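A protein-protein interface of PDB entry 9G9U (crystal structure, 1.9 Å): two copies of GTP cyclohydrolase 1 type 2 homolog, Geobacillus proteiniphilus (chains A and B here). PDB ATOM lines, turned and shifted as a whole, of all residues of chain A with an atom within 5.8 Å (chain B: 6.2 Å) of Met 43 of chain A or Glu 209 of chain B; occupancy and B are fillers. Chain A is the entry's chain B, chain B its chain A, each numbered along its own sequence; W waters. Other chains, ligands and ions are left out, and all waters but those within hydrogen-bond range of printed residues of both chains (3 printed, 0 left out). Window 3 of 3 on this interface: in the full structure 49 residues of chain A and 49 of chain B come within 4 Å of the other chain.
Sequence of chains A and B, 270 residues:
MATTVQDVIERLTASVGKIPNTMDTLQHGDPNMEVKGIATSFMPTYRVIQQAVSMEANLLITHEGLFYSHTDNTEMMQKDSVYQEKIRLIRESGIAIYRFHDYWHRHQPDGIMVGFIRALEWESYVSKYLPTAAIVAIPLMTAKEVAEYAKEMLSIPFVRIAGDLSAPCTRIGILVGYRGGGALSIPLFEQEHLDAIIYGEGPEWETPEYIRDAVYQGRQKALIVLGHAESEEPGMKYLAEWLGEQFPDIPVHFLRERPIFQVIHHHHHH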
ATOM      1  N   SER A  41     -10.846  35.285  -4.083  1.00  0.00           N
ATOM      2  CA  SER A  41     -12.139  34.649  -3.888  1.00  0.00           C
ATOM      3  C   SER A  41     -12.872  35.369  -2.769  1.00  0.00           C
ATOM      4  O   SER A  41     -12.265  36.047  -1.943  1.00  0.00           O
ATOM      5  CB  SER A  41     -11.984  33.148  -3.554  1.00  0.00           C
ATOM      6  OG  SER A  41     -11.867  32.938  -2.159  1.00  0.00           O
ATOM      7  N   PHE A  42     -14.194  35.244  -2.760  1.00  0.00           N
ATOM      8  CA  PHE A  42     -14.938  35.717  -1.600  1.00  0.00           C
ATOM      9  C   PHE A  42     -14.665  34.820  -0.402  1.00  0.00           C
ATOM     10  O   PHE A  42     -14.290  35.289   0.680  1.00  0.00           O
ATOM     11  CB  PHE A  42     -16.441  35.757  -1.912  1.00  0.00           C
ATOM     12  CG  PHE A  42     -17.309  35.979  -0.695  1.00  0.00           C
ATOM     13  CD1 PHE A  42     -17.331  37.207  -0.044  1.00  0.00           C
ATOM     14  CD2 PHE A  42     -18.115  34.958  -0.218  1.00  0.00           C
ATOM     15  CE1 PHE A  42     -18.148  37.411   1.082  1.00  0.00           C
ATOM     16  CE2 PHE A  42     -18.930  35.155   0.902  1.00  0.00           C
ATOM     17  CZ  PHE A  42     -18.943  36.378   1.551  1.00  0.00           C
ATOM     18  N   MET A  43     -14.831  33.519  -0.589  1.00  0.00           N
ATOM     19  CA  MET A  43     -14.761  32.519   0.448  1.00  0.00           C
ATOM     20  C   MET A  43     -13.686  31.496   0.095  1.00  0.00           C
ATOM     21  O   MET A  43     -13.593  31.069  -1.062  1.00  0.00           O
ATOM     22  CB  MET A  43     -16.132  31.848   0.584  1.00  0.00           C
ATOM     23  CG  MET A  43     -16.254  30.767   1.628  1.00  0.00           C
ATOM     24  SD  MET A  43     -16.534  31.492   3.240  1.00  0.00           S
ATOM     25  CE  MET A  43     -17.837  32.670   2.881  1.00  0.00           C
ATOM     26  N   PRO A  44     -12.842  31.128   1.037  1.00  0.00           N
ATOM     27  CA  PRO A  44     -11.793  30.122   0.746  1.00  0.00           C
ATOM     28  C   PRO A  44     -12.336  28.704   0.831  1.00  0.00           C
ATOM     29  O   PRO A  44     -11.951  27.901   1.680  1.00  0.00           O
ATOM     30  CB  PRO A  44     -10.745  30.419   1.822  1.00  0.00           C
ATOM     31  CG  PRO A  44     -11.547  30.938   2.974  1.00  0.00           C
ATOM     32  CD  PRO A  44     -12.706  31.705   2.390  1.00  0.00           C
ATOM     33  N   THR A  45     -13.275  28.378  -0.059  1.00  0.00           N
ATOM     34  CA  THR A  45     -13.894  27.069   0.032  1.00  0.00           C
ATOM     35  C   THR A  45     -12.872  25.980  -0.277  1.00  0.00           C
ATOM     36  O   THR A  45     -11.776  26.237  -0.793  1.00  0.00           O
ATOM     37  CB  THR A  45     -15.076  26.946  -0.919  1.00  0.00           C
ATOM     38  OG1 THR A  45     -14.579  26.775  -2.246  1.00  0.00           O
ATOM     39  CG2 THR A  45     -15.983  28.241  -0.848  1.00  0.00           C
ATOM     40  N   VAL A  48     -12.320  26.112  -3.935  1.00  0.00           N
ATOM     41  CA  VAL A  48     -11.504  27.267  -4.310  1.00  0.00           C
ATOM     42  C   VAL A  48     -10.025  26.961  -4.104  1.00  0.00           C
ATOM     43  O   VAL A  48      -9.183  27.299  -4.947  1.00  0.00           O
ATOM     44  CB  VAL A  48     -11.936  28.523  -3.524  1.00  0.00           C
ATOM     45  CG1 VAL A  48     -10.821  29.570  -3.528  1.00  0.00           C
ATOM     46  CG2 VAL A  48     -13.200  29.115  -4.114  1.00  0.00           C
ATOM     47  N   THR A  62      -8.547  36.051   0.021  1.00  0.00           N
ATOM     48  CA  THR A  62      -9.964  35.794   0.204  1.00  0.00           C
ATOM     49  C   THR A  62     -10.518  36.770   1.236  1.00  0.00           C
ATOM     50  O   THR A  62      -9.780  37.356   2.036  1.00  0.00           O
ATOM     51  CB  THR A  62     -10.184  34.339   0.625  1.00  0.00           C
ATOM     52  OG1 THR A  62     -11.547  33.976   0.398  1.00  0.00           O
ATOM     53  CG2 THR A  62      -9.857  34.160   2.090  1.00  0.00           C
ATOM     54  N   HIS A  63     -11.833  36.979   1.182  1.00  0.00           N
ATOM     55  CA  HIS A  63     -12.469  37.958   2.048  1.00  0.00           C
ATOM     56  C   HIS A  63     -12.851  37.384   3.407  1.00  0.00           C
ATOM     57  O   HIS A  63     -12.836  38.112   4.405  1.00  0.00           O
ATOM     58  CB  HIS A  63     -13.712  38.527   1.350  1.00  0.00           C
ATOM     59  CG  HIS A  63     -14.260  39.766   1.987  1.00  0.00           C
ATOM     60  ND1 HIS A  63     -13.583  40.971   1.993  1.00  0.00           N
ATOM     61  CD2 HIS A  63     -15.443  39.998   2.606  1.00  0.00           C
ATOM     62  CE1 HIS A  63     -14.320  41.882   2.603  1.00  0.00           C
ATOM     63  NE2 HIS A  63     -15.451  41.316   2.987  1.00  0.00           N
ATOM     64  N   GLU A  64     -13.141  36.089   3.479  1.00  0.00           N
ATOM     65  CA  GLU A  64     -13.743  35.474   4.650  1.00  0.00           C
ATOM     66  C   GLU A  64     -12.808  34.426   5.239  1.00  0.00           C
ATOM     67  O   GLU A  64     -11.761  34.104   4.676  1.00  0.00           O
ATOM     68  CB  GLU A  64     -15.094  34.845   4.290  1.00  0.00           C
ATOM     69  CG  GLU A  64     -16.125  35.870   3.833  1.00  0.00           C
ATOM     70  CD  GLU A  64     -16.677  36.706   4.982  1.00  0.00           C
ATOM     71  OE1 GLU A  64     -17.068  37.869   4.758  1.00  0.00           O
ATOM     72  OE2 GLU A  64     -16.737  36.204   6.112  1.00  0.00           O
ATOM     73  N   GLY A  65     -13.208  33.888   6.388  1.00  0.00           N
ATOM     74  CA  GLY A  65     -12.352  32.978   7.119  1.00  0.00           C
ATOM     75  C   GLY A  65     -12.388  31.578   6.551  1.00  0.00           C
ATOM     76  O   GLY A  65     -13.200  31.242   5.687  1.00  0.00           O
ATOM     77  N   TYR A  68     -15.736  28.732   8.525  1.00  0.00           N
ATOM     78  CA  TYR A  68     -17.172  28.928   8.701  1.00  0.00           C
ATOM     79  C   TYR A  68     -17.476  29.824   9.886  1.00  0.00           C
ATOM     80  O   TYR A  68     -18.492  29.663  10.573  1.00  0.00           O
ATOM     81  CB  TYR A  68     -17.883  27.583   8.836  1.00  0.00           C
ATOM     82  CG  TYR A  68     -17.166  26.519   8.039  1.00  0.00           C
ATOM     83  CD1 TYR A  68     -16.971  26.670   6.672  1.00  0.00           C
ATOM     84  CD2 TYR A  68     -16.655  25.385   8.658  1.00  0.00           C
ATOM     85  CE1 TYR A  68     -16.284  25.702   5.933  1.00  0.00           C
ATOM     86  CE2 TYR A  68     -15.980  24.416   7.940  1.00  0.00           C
ATOM     87  CZ  TYR A  68     -15.797  24.570   6.587  1.00  0.00           C
ATOM     88  OH  TYR A  68     -15.111  23.569   5.932  1.00  0.00           O
ATOM     89  N   ALA A 229     -22.501  36.596  -0.324  1.00  0.00           N
ATOM     90  CA  ALA A 229     -21.510  36.415  -1.389  1.00  0.00           C
ATOM     91  C   ALA A 229     -21.873  37.225  -2.626  1.00  0.00           C
ATOM     92  O   ALA A 229     -21.000  37.780  -3.299  1.00  0.00           O
ATOM     93  CB  ALA A 229     -21.379  34.931  -1.757  1.00  0.00           C
ATOM     94  N   GLU A 257     -17.527  31.335  -7.048  1.00  0.00           N
ATOM     95  CA  GLU A 257     -18.106  30.137  -6.477  1.00  0.00           C
ATOM     96  C   GLU A 257     -19.571  30.043  -6.894  1.00  0.00           C
ATOM     97  O   GLU A 257     -20.137  30.983  -7.456  1.00  0.00           O
ATOM     98  CB  GLU A 257     -17.979  30.140  -4.949  1.00  0.00           C
ATOM     99  CG  GLU A 257     -16.883  29.232  -4.406  1.00  0.00           C
ATOM    100  CD  GLU A 257     -17.222  27.763  -4.482  1.00  0.00           C
ATOM    101  OE1 GLU A 257     -18.273  27.417  -5.070  1.00  0.00           O
ATOM    102  OE2 GLU A 257     -16.430  26.950  -3.933  1.00  0.00           O
ATOM    103  N   ILE A 260     -24.722  29.809  -2.797  1.00  0.00           N
ATOM    104  CA  ILE A 260     -24.821  28.924  -1.648  1.00  0.00           C
ATOM    105  C   ILE A 260     -26.192  28.259  -1.599  1.00  0.00           C
ATOM    106  O   ILE A 260     -26.308  27.088  -1.222  1.00  0.00           O
ATOM    107  CB  ILE A 260     -24.518  29.699  -0.355  1.00  0.00           C
ATOM    108  CG1 ILE A 260     -24.355  28.711   0.790  1.00  0.00           C
ATOM    109  CG2 ILE A 260     -25.599  30.746  -0.044  1.00  0.00           C
ATOM    110  CD1 ILE A 260     -23.230  27.724   0.563  1.00  0.00           C
ATOM    111  N   GLU B 204     -25.064  33.594   6.601  1.00  0.00           N
ATOM    112  CA  GLU B 204     -24.780  32.848   5.383  1.00  0.00           C
ATOM    113  C   GLU B 204     -23.363  32.292   5.351  1.00  0.00           C
ATOM    114  O   GLU B 204     -23.114  31.324   4.631  1.00  0.00           O
ATOM    115  CB  GLU B 204     -25.004  33.737   4.142  1.00  0.00           C
ATOM    116  CG  GLU B 204     -26.479  34.016   3.969  1.00  0.00           C
ATOM    117  CD  GLU B 204     -26.826  34.821   2.736  1.00  0.00           C
ATOM    118  OE1 GLU B 204     -26.007  34.885   1.807  1.00  0.00           O
ATOM    119  OE2 GLU B 204     -27.955  35.369   2.710  1.00  0.00           O
ATOM    120  N   TRP B 205     -22.439  32.875   6.103  1.00  0.00           N
ATOM    121  CA  TRP B 205     -21.039  32.507   5.997  1.00  0.00           C
ATOM    122  C   TRP B 205     -20.625  31.434   6.993  1.00  0.00           C
ATOM    123  O   TRP B 205     -19.431  31.105   7.063  1.00  0.00           O
ATOM    124  CB  TRP B 205     -20.154  33.759   6.179  1.00  0.00           C
ATOM    125  CG  TRP B 205     -20.231  34.377   7.540  1.00  0.00           C
ATOM    126  CD1 TRP B 205     -19.396  34.139   8.594  1.00  0.00           C
ATOM    127  CD2 TRP B 205     -21.215  35.314   8.010  1.00  0.00           C
ATOM    128  NE1 TRP B 205     -19.799  34.869   9.690  1.00  0.00           N
ATOM    129  CE2 TRP B 205     -20.909  35.602   9.358  1.00  0.00           C
ATOM    130  CE3 TRP B 205     -22.320  35.935   7.421  1.00  0.00           C
ATOM    131  CZ2 TRP B 205     -21.661  36.495  10.124  1.00  0.00           C
ATOM    132  CZ3 TRP B 205     -23.075  36.824   8.187  1.00  0.00           C
ATOM    133  CH2 TRP B 205     -22.741  37.090   9.527  1.00  0.00           C
ATOM    134  N   GLU B 206     -21.573  30.857   7.756  1.00  0.00           N
ATOM    135  CA  GLU B 206     -21.239  29.889   8.782  1.00  0.00           C
ATOM    136  C   GLU B 206     -21.775  28.525   8.325  1.00  0.00           C
ATOM    137  O   GLU B 206     -21.149  27.892   7.458  1.00  0.00           O
ATOM    138  CB  GLU B 206     -21.776  30.340  10.145  1.00  0.00           C
ATOM    139  CG  GLU B 206     -21.055  31.561  10.713  1.00  0.00           C
ATOM    140  CD  GLU B 206     -21.589  32.006  12.082  1.00  0.00           C
ATOM    141  OE1 GLU B 206     -22.574  31.419  12.572  1.00  0.00           O
ATOM    142  OE2 GLU B 206     -21.023  32.964  12.657  1.00  0.00           O
ATOM    143  N   THR B 207     -22.912  28.060   8.856  1.00  0.00           N
ATOM    144  CA  THR B 207     -23.370  26.700   8.555  1.00  0.00           C
ATOM    145  C   THR B 207     -23.512  26.409   7.067  1.00  0.00           C
ATOM    146  O   THR B 207     -23.117  25.306   6.657  1.00  0.00           O
ATOM    147  CB  THR B 207     -24.688  26.410   9.292  1.00  0.00           C
ATOM    148  OG1 THR B 207     -24.553  26.763  10.685  1.00  0.00           O
ATOM    149  CG2 THR B 207     -25.040  24.935   9.221  1.00  0.00           C
ATOM    150  N   PRO B 208     -24.018  27.309   6.210  1.00  0.00           N
ATOM    151  CA  PRO B 208     -24.094  26.946   4.779  1.00  0.00           C
ATOM    152  C   PRO B 208     -22.731  26.724   4.155  1.00  0.00           C
ATOM    153  O   PRO B 208     -22.612  25.896   3.249  1.00  0.00           O
ATOM    154  CB  PRO B 208     -24.823  28.141   4.143  1.00  0.00           C
ATOM    155  CG  PRO B 208     -25.559  28.806   5.305  1.00  0.00           C
ATOM    156  CD  PRO B 208     -24.595  28.643   6.463  1.00  0.00           C
ATOM    157  N   GLU B 209     -21.689  27.432   4.610  1.00  0.00           N
ATOM    158  CA  GLU B 209     -20.358  27.214   4.053  1.00  0.00           C
ATOM    159  C   GLU B 209     -19.760  25.908   4.548  1.00  0.00           C
ATOM    160  O   GLU B 209     -19.005  25.249   3.824  1.00  0.00           O
ATOM    161  CB  GLU B 209     -19.442  28.379   4.410  1.00  0.00           C
ATOM    162  CG  GLU B 209     -19.846  29.649   3.701  1.00  0.00           C
ATOM    163  CD  GLU B 209     -19.666  29.559   2.195  1.00  0.00           C
ATOM    164  OE1 GLU B 209     -18.976  28.624   1.726  1.00  0.00           O
ATOM    165  OE2 GLU B 209     -20.206  30.435   1.474  1.00  0.00           O
ATOM    166  N   TYR B 210     -20.070  25.530   5.789  1.00  0.00           N
ATOM    167  CA  TYR B 210     -19.714  24.201   6.264  1.00  0.00           C
ATOM    168  C   TYR B 210     -20.320  23.132   5.370  1.00  0.00           C
ATOM    169  O   TYR B 210     -19.627  22.204   4.926  1.00  0.00           O
ATOM    170  CB  TYR B 210     -20.154  24.046   7.715  1.00  0.00           C
ATOM    171  CG  TYR B 210     -20.083  22.615   8.227  1.00  0.00           C
ATOM    172  CD1 TYR B 210     -18.882  22.069   8.689  1.00  0.00           C
ATOM    173  CD2 TYR B 210     -21.214  21.820   8.259  1.00  0.00           C
ATOM    174  CE1 TYR B 210     -18.828  20.757   9.165  1.00  0.00           C
ATOM    175  CE2 TYR B 210     -21.170  20.520   8.730  1.00  0.00           C
ATOM    176  CZ  TYR B 210     -19.976  19.986   9.181  1.00  0.00           C
ATOM    177  OH  TYR B 210     -19.964  18.675   9.645  1.00  0.00           O
ATOM    178  N   ILE B 211     -21.601  23.278   5.039  1.00  0.00           N
ATOM    179  CA  ILE B 211     -22.260  22.277   4.206  1.00  0.00           C
ATOM    180  C   ILE B 211     -21.688  22.286   2.792  1.00  0.00           C
ATOM    181  O   ILE B 211     -21.502  21.222   2.181  1.00  0.00           O
ATOM    182  CB  ILE B 211     -23.784  22.498   4.210  1.00  0.00           C
ATOM    183  CG1 ILE B 211     -24.381  22.001   5.535  1.00  0.00           C
ATOM    184  CG2 ILE B 211     -24.427  21.791   3.033  1.00  0.00           C
ATOM    185  CD1 ILE B 211     -24.122  20.510   5.837  1.00  0.00           C
ATOM    186  N   ARG B 212     -21.362  23.477   2.256  1.00  0.00           N
ATOM    187  CA  ARG B 212     -20.742  23.545   0.932  1.00  0.00           C
ATOM    188  C   ARG B 212     -19.472  22.706   0.879  1.00  0.00           C
ATOM    189  O   ARG B 212     -19.261  21.922  -0.056  1.00  0.00           O
ATOM    190  CB  ARG B 212     -20.420  24.995   0.563  1.00  0.00           C
ATOM    191  CG  ARG B 212     -20.099  25.154  -0.913  1.00  0.00           C
ATOM    192  CD  ARG B 212     -19.105  26.251  -1.130  1.00  0.00           C
ATOM    193  NE  ARG B 212     -19.617  27.597  -0.840  1.00  0.00           N
ATOM    194  CZ  ARG B 212     -20.304  28.357  -1.699  1.00  0.00           C
ATOM    195  NH1 ARG B 212     -20.627  27.914  -2.904  1.00  0.00           N
ATOM    196  NH2 ARG B 212     -20.676  29.578  -1.340  1.00  0.00           N
ATOM    197  N   ASP B 213     -18.603  22.883   1.870  1.00  0.00           N
ATOM    198  CA  ASP B 213     -17.357  22.117   1.923  1.00  0.00           C
ATOM    199  C   ASP B 213     -17.616  20.639   2.142  1.00  0.00           C
ATOM    200  O   ASP B 213     -16.960  19.796   1.511  1.00  0.00           O
ATOM    201  CB  ASP B 213     -16.457  22.643   3.034  1.00  0.00           C
ATOM    202  CG  ASP B 213     -15.587  23.781   2.578  1.00  0.00           C
ATOM    203  OD1 ASP B 213     -15.639  24.169   1.392  1.00  0.00           O
ATOM    204  OD2 ASP B 213     -14.854  24.302   3.423  1.00  0.00           O
ATOM    205  N   ALA B 214     -18.538  20.302   3.054  1.00  0.00           N
ATOM    206  CA  ALA B 214     -18.845  18.897   3.306  1.00  0.00           C
ATOM    207  C   ALA B 214     -19.279  18.204   2.021  1.00  0.00           C
ATOM    208  O   ALA B 214     -18.819  17.097   1.711  1.00  0.00           O
ATOM    209  CB  ALA B 214     -19.931  18.773   4.386  1.00  0.00           C
ATOM    210  N   LEU B 223     -28.859  21.558   3.869  1.00  0.00           N
ATOM    211  CA  LEU B 223     -29.372  22.528   4.811  1.00  0.00           C
ATOM    212  C   LEU B 223     -30.617  23.143   4.192  1.00  0.00           C
ATOM    213  O   LEU B 223     -30.577  23.583   3.040  1.00  0.00           O
ATOM    214  CB  LEU B 223     -28.301  23.601   5.093  1.00  0.00           C
ATOM    215  CG  LEU B 223     -28.566  24.678   6.132  1.00  0.00           C
ATOM    216  CD1 LEU B 223     -28.701  24.109   7.556  1.00  0.00           C
ATOM    217  CD2 LEU B 223     -27.436  25.718   6.040  1.00  0.00           C
HETATM  218  O   HOH W   1     -20.591  24.976  -4.170  1.00  0.00           O
HETATM  219  O   HOH W   2     -16.925  31.818   6.455  1.00  0.00           O
HETATM  220  O   HOH W   3     -23.666  33.949   0.507  1.00  0.00           O
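NH1 of Arg 212 of chain B lies within salt-bridge range of OE1 of Glu 257 of chain A. The side-chain hydroxyl of Tyr 68 of chain A lies within hydrogen-bond range of the side-chain carboxylate of Asp 213 of chain B, 2.6 Å away.
Water W2 bridges O of Trp 205 of chain B (2.7 Å) and SD of Met 43 of chain A (3.3 Å). Water W3 lies within hydrogen-bond range of OE1 of Glu 204 of chain B (2.8 Å) and N of Ala 229 of chain A (3.0 Å). Water W1 bridges the guanidinium group (NH1) of Arg 212 of chain B (3.2 Å) and the side-chain carboxylate (OE1) of Glu 257 of chain A (3.5 Å).
Of chain A, only Met 43, Thr 45 and Tyr 68 come within 4 Å of Glu 209 of chain B. Of the printed residues of chain B, Glu 257 of chain A touches Arg 212 (3.2 Å). Of the printed residues of chain A, Tyr 210 of chain B touches Tyr 68 (3.4 Å). Glu 64 of chain A touches none of the printed residues of chain B. Val 48 of chain A touches none of the printed residues of chain B. The nearest residue of chain B that does not touch Met 43 of chain A is Trp 205 of chain B (4.2 Å). The nearest residue of chain A that does not touch Glu 209 of chain B is Ile 260 of chain A (4.2 Å). The nearest printed residue of chain B that does not touch Ile 260 of chain A is Glu 209 of chain B (4.2 Å).
Of the 12 printed residues of chain B, 7 touch a printed residue of chain A. Of the 14 printed residues of chain A, 5 touch a printed residue of chain B. Printed residues of chain A that touch a printed residue of chain B: Met 43, Thr 45, Tyr 68, Glu 257 and Ile 260. Among the printed residues, Asp or Glu carboxylates within 4 Å of a Lys or Arg side-chain nitrogen of the other chain: Glu 257 of chain A with Arg 212 of chain B (3.2 Å).
No position is printed for both chains. Of the 12 pairs that touch across the chains among the printed residues, none has its exchanged pair printed and touching as well.
Among the printed residues, merely in contact across the chains: Met 43 of chain A with Glu 209 of chain B (3.5 Å), Thr 45 of chain A with Glu 209 of chain B (3.97 Å), Thr 45 of chain A with Arg 212 of chain B (3.7 Å), Thr 45 of chain A with Asp 213 of chain B (3.6 Å), Tyr 68 of chain A with Trp 205 of chain B (3.5 Å), Tyr 68 of chain A with Glu 206 of chain B (3.2 Å), Tyr 68 of chain A with Glu 209 of chain B (3.5 Å), Tyr 68 of chain A with Tyr 210 of chain B (3.4 Å), Ile 260 of chain A with Pro 208 of chain B (3.3 Å) and Ile 260 of chain A with Arg 212 of chain B (3.7 Å).
N of Val 48 of chain A sits at hydrogen-bond distance from OG1 of Thr 45 of chain A. OG1 of Thr 45 of chain A sits at hydrogen-bond distance from OE2 of Glu 257 of chain A (2.5 Å). The side-chain hydroxyl (OG) of Ser 41 of chain A lies within hydrogen-bond range of the backbone carbonyl oxygen (O) of Met 43 of chain A (2.8 Å). The side-chain carboxylate of Glu 209 of chain B lies within salt-bridge range of the guanidinium group of Arg 212 of chain B, 2.8 Å away. OG1 of Thr 62 of chain A lies close to N of Met 43 of chain A (3.5 Å).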
